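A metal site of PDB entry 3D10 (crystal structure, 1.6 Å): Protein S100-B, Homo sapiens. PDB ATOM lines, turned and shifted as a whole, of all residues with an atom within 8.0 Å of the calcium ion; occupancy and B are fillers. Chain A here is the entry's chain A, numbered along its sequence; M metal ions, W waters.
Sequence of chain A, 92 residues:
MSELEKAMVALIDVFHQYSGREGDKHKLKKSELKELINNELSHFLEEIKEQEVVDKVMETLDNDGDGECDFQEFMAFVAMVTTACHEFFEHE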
ATOM      1  N   LYS A  27      -7.372 -25.769   5.515  1.00  0.00           N
ATOM      2  CA  LYS A  27      -6.577 -26.536   4.577  1.00  0.00           C
ATOM      3  C   LYS A  27      -5.739 -27.550   5.303  1.00  0.00           C
ATOM      4  O   LYS A  27      -5.284 -27.224   6.401  1.00  0.00           O
ATOM      5  CB  LYS A  27      -5.674 -25.636   3.722  1.00  0.00           C
ATOM      6  CG  LYS A  27      -6.378 -24.552   2.862  1.00  0.00           C
ATOM      7  CD  LYS A  27      -5.406 -24.153   1.739  1.00  0.00           C
ATOM      8  CE  LYS A  27      -5.441 -22.668   1.442  1.00  0.00           C
ATOM      9  NZ  LYS A  27      -6.708 -22.207   0.823  1.00  0.00           N
ATOM     10  N   LEU A  28      -5.505 -28.722   4.673  1.00  0.00           N
ATOM     11  CA  LEU A  28      -4.581 -29.758   5.178  1.00  0.00           C
ATOM     12  C   LEU A  28      -3.151 -29.490   4.735  1.00  0.00           C
ATOM     13  O   LEU A  28      -2.870 -29.521   3.569  1.00  0.00           O
ATOM     14  CB  LEU A  28      -4.954 -31.174   4.660  1.00  0.00           C
ATOM     15  CG  LEU A  28      -6.309 -31.673   5.136  1.00  0.00           C
ATOM     16  CD1 LEU A  28      -6.842 -32.862   4.274  1.00  0.00           C
ATOM     17  CD2 LEU A  28      -6.435 -31.971   6.656  1.00  0.00           C
ATOM     18  N   MET A  58       0.445 -35.476  -1.288  1.00  0.00           N
ATOM     19  CA  MET A  58       0.211 -34.046  -1.484  1.00  0.00           C
ATOM     20  C   MET A  58       0.357 -33.613  -2.934  1.00  0.00           C
ATOM     21  O   MET A  58      -0.575 -33.072  -3.432  1.00  0.00           O
ATOM     22  CB  MET A  58       1.090 -33.184  -0.574  1.00  0.00           C
ATOM     23  CG  MET A  58       0.613 -31.713  -0.596  1.00  0.00           C
ATOM     24  SD  MET A  58      -1.028 -31.536   0.099  1.00  0.00           S
ATOM     25  CE  MET A  58      -0.715 -31.468   1.879  1.00  0.00           C
ATOM     26  N   LEU A  61      -2.663 -34.672  -4.911  1.00  0.00           N
ATOM     27  CA  LEU A  61      -3.982 -34.076  -4.749  1.00  0.00           C
ATOM     28  C   LEU A  61      -4.019 -32.535  -4.892  1.00  0.00           C
ATOM     29  O   LEU A  61      -5.112 -31.951  -5.061  1.00  0.00           O
ATOM     30  CB  LEU A  61      -4.691 -34.598  -3.474  1.00  0.00           C
ATOM     31  CG  LEU A  61      -3.999 -34.540  -2.137  1.00  0.00           C
ATOM     32  CD1 LEU A  61      -3.693 -33.079  -1.745  1.00  0.00           C
ATOM     33  CD2 LEU A  61      -4.816 -35.299  -1.052  1.00  0.00           C
ATOM     34  N   ASP A  62      -2.860 -31.916  -4.844  1.00  0.00           N
ATOM     35  CA  ASP A  62      -2.774 -30.458  -4.807  1.00  0.00           C
ATOM     36  C   ASP A  62      -2.863 -29.819  -6.183  1.00  0.00           C
ATOM     37  O   ASP A  62      -1.856 -29.575  -6.854  1.00  0.00           O
ATOM     38  CB  ASP A  62      -1.520 -29.981  -4.041  1.00  0.00           C
ATOM     39  CG  ASP A  62      -1.374 -28.468  -4.023  1.00  0.00           C
ATOM     40  OD1 ASP A  62      -2.432 -27.772  -4.080  1.00  0.00           O
ATOM     41  OD2 ASP A  62      -0.212 -27.984  -3.930  1.00  0.00           O
ATOM     42  N   ASN A  63      -4.079 -29.448  -6.561  1.00  0.00           N
ATOM     43  CA  ASN A  63      -4.333 -28.974  -7.905  1.00  0.00           C
ATOM     44  C   ASN A  63      -4.046 -27.504  -8.130  1.00  0.00           C
ATOM     45  O   ASN A  63      -3.786 -27.086  -9.255  1.00  0.00           O
ATOM     46  CB  ASN A  63      -5.779 -29.293  -8.258  1.00  0.00           C
ATOM     47  CG  ASN A  63      -6.006 -30.773  -8.437  1.00  0.00           C
ATOM     48  OD1 ASN A  63      -7.088 -31.287  -8.156  1.00  0.00           O
ATOM     49  ND2 ASN A  63      -4.963 -31.492  -8.904  1.00  0.00           N
ATOM     50  N   ASP A  64      -4.110 -26.715  -7.069  1.00  0.00           N
ATOM     51  CA  ASP A  64      -3.837 -25.282  -7.163  1.00  0.00           C
ATOM     52  C   ASP A  64      -2.400 -24.913  -6.709  1.00  0.00           C
ATOM     53  O   ASP A  64      -2.029 -23.727  -6.673  1.00  0.00           O
ATOM     54  CB  ASP A  64      -4.903 -24.462  -6.437  1.00  0.00           C
ATOM     55  CG  ASP A  64      -4.890 -24.692  -4.944  1.00  0.00           C
ATOM     56  OD1 ASP A  64      -5.709 -24.090  -4.245  1.00  0.00           O
ATOM     57  OD2 ASP A  64      -4.063 -25.480  -4.474  1.00  0.00           O
ATOM     58  N   GLY A  65      -1.625 -25.924  -6.363  1.00  0.00           N
ATOM     59  CA  GLY A  65      -0.205 -25.756  -6.065  1.00  0.00           C
ATOM     60  C   GLY A  65       0.209 -24.905  -4.878  1.00  0.00           C
ATOM     61  O   GLY A  65       1.363 -24.462  -4.829  1.00  0.00           O
ATOM     62  N   ASP A  66      -0.684 -24.660  -3.924  1.00  0.00           N
ATOM     63  CA  ASP A  66      -0.299 -23.928  -2.696  1.00  0.00           C
ATOM     64  C   ASP A  66       0.350 -24.893  -1.652  1.00  0.00           C
ATOM     65  O   ASP A  66       0.595 -24.545  -0.493  1.00  0.00           O
ATOM     66  CB  ASP A  66      -1.505 -23.139  -2.114  1.00  0.00           C
ATOM     67  CG  ASP A  66      -2.614 -24.062  -1.547  1.00  0.00           C
ATOM     68  OD1 ASP A  66      -2.557 -25.271  -1.822  1.00  0.00           O
ATOM     69  OD2 ASP A  66      -3.541 -23.574  -0.852  1.00  0.00           O
ATOM     70  N   GLY A  67       0.663 -26.107  -2.067  1.00  0.00           N
ATOM     71  CA  GLY A  67       1.256 -27.069  -1.140  1.00  0.00           C
ATOM     72  C   GLY A  67       0.348 -27.537  -0.021  1.00  0.00           C
ATOM     73  O   GLY A  67       0.808 -28.171   0.927  1.00  0.00           O
ATOM     74  N   GLU A  68      -0.949 -27.280  -0.156  1.00  0.00           N
ATOM     75  CA  GLU A  68      -1.903 -27.731   0.845  1.00  0.00           C
ATOM     76  C   GLU A  68      -3.124 -28.369   0.162  1.00  0.00           C
ATOM     77  O   GLU A  68      -3.376 -28.220  -1.023  1.00  0.00           O
ATOM     78  CB  GLU A  68      -2.362 -26.587   1.768  1.00  0.00           C
ATOM     79  CG  GLU A  68      -1.208 -25.837   2.450  1.00  0.00           C
ATOM     80  CD  GLU A  68      -1.436 -25.556   3.917  1.00  0.00           C
ATOM     81  OE1 GLU A  68      -2.413 -26.069   4.538  1.00  0.00           O
ATOM     82  OE2 GLU A  68      -0.558 -24.844   4.464  1.00  0.00           O
ATOM     83  N   CYS A  69      -3.878 -29.099   0.922  1.00  0.00           N
ATOM     84  CA  CYS A  69      -5.098 -29.724   0.397  1.00  0.00           C
ATOM     85  C   CYS A  69      -6.297 -28.959   0.924  1.00  0.00           C
ATOM     86  O   CYS A  69      -6.524 -28.977   2.151  1.00  0.00           O
ATOM     87  CB  CYS A  69      -5.225 -31.143   0.950  1.00  0.00           C
ATOM     88  SG  CYS A  69      -6.557 -32.095   0.241  1.00  0.00           S
ATOM     89  N   ASP A  70      -7.084 -28.330   0.058  1.00  0.00           N
ATOM     90  CA  ASP A  70      -8.281 -27.624   0.570  1.00  0.00           C
ATOM     91  C   ASP A  70      -9.487 -28.523   0.541  1.00  0.00           C
ATOM     92  O   ASP A  70      -9.370 -29.712   0.253  1.00  0.00           O
ATOM     93  CB  ASP A  70      -8.514 -26.294  -0.165  1.00  0.00           C
ATOM     94  CG  ASP A  70      -8.774 -26.478  -1.657  1.00  0.00           C
ATOM     95  OD1 ASP A  70      -9.066 -27.607  -2.152  1.00  0.00           O
ATOM     96  OD2 ASP A  70      -8.732 -25.454  -2.366  1.00  0.00           O
ATOM     97  N   PHE A  71     -10.668 -28.031   0.928  1.00  0.00           N
ATOM     98  CA  PHE A  71     -11.825 -28.924   0.888  1.00  0.00           C
ATOM     99  C   PHE A  71     -12.123 -29.594  -0.487  1.00  0.00           C
ATOM    100  O   PHE A  71     -12.365 -30.779  -0.585  1.00  0.00           O
ATOM    101  CB  PHE A  71     -13.095 -28.186   1.407  1.00  0.00           C
ATOM    102  CG  PHE A  71     -14.274 -29.048   1.454  1.00  0.00           C
ATOM    103  CD1 PHE A  71     -14.437 -29.934   2.527  1.00  0.00           C
ATOM    104  CD2 PHE A  71     -15.212 -29.051   0.436  1.00  0.00           C
ATOM    105  CE1 PHE A  71     -15.541 -30.816   2.561  1.00  0.00           C
ATOM    106  CE2 PHE A  71     -16.306 -29.919   0.469  1.00  0.00           C
ATOM    107  CZ  PHE A  71     -16.468 -30.792   1.537  1.00  0.00           C
ATOM    108  N   GLU A  73     -10.080 -30.164  -2.920  1.00  0.00           N
ATOM    109  CA  GLU A  73      -9.068 -31.206  -3.134  1.00  0.00           C
ATOM    110  C   GLU A  73      -9.231 -32.459  -2.263  1.00  0.00           C
ATOM    111  O   GLU A  73      -9.012 -33.612  -2.703  1.00  0.00           O
ATOM    112  CB  GLU A  73      -7.688 -30.585  -2.920  1.00  0.00           C
ATOM    113  CG  GLU A  73      -7.292 -29.616  -4.056  1.00  0.00           C
ATOM    114  CD  GLU A  73      -6.226 -28.649  -3.632  1.00  0.00           C
ATOM    115  OE1 GLU A  73      -5.884 -28.476  -2.428  1.00  0.00           O
ATOM    116  OE2 GLU A  73      -5.750 -27.917  -4.487  1.00  0.00           O
ATOM    117  N   PHE A  74      -9.674 -32.254  -1.028  1.00  0.00           N
ATOM    118  CA  PHE A  74     -10.009 -33.341  -0.203  1.00  0.00           C
ATOM    119  C   PHE A  74     -11.179 -34.193  -0.761  1.00  0.00           C
ATOM    120  O   PHE A  74     -11.143 -35.430  -0.776  1.00  0.00           O
ATOM    121  CB  PHE A  74     -10.359 -32.828   1.188  1.00  0.00           C
ATOM    122  CG  PHE A  74     -10.646 -33.963   2.224  1.00  0.00           C
ATOM    123  CD1 PHE A  74      -9.630 -34.887   2.537  1.00  0.00           C
ATOM    124  CD2 PHE A  74     -11.903 -34.150   2.755  1.00  0.00           C
ATOM    125  CE1 PHE A  74      -9.908 -35.916   3.460  1.00  0.00           C
ATOM    126  CE2 PHE A  74     -12.183 -35.170   3.682  1.00  0.00           C
ATOM    127  CZ  PHE A  74     -11.190 -36.060   4.035  1.00  0.00           C
HETATM  128 CA    CA M   1      -4.035 -26.926  -2.724  1.00  0.00          CA
HETATM  129  O   HOH W   1      -5.525 -25.468  -1.737  1.00  0.00           O
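OD2 of Asp 62 sits close to N of Gly 65. The side-chain carboxylate of Asp 62 is in hydrogen-bond range of the backbone NH of Gly 67 (2.8 Å). The side-chain carboxylate of Asp 66 lies within salt-bridge range of the side-chain amino group of Lys 27 (3.8 Å). The backbone NH (N) of Glu 73 sits at hydrogen-bond distance from the side-chain carboxylate (OD1) of Asp 70 (2.9 Å). OE2 of Glu 73 lies close to N of Asn 63.
The calcium ion is bound by the backbone carbonyl oxygen (O) of Glu 68 (2.2 Å), the side-chain carboxylate (OD1) of Asp 62 (2.3 Å), the side-chain carboxylate (OD2) of Asp 64 (2.3 Å), water W1 (2.3 Å), the side-chain carboxylate (OD1) of Asp 66 (2.4 Å), the side-chain carboxylate (OE1) of Glu 73 (2.4 Å) and the side-chain carboxylate (OE2) of Glu 73 (2.7 Å).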
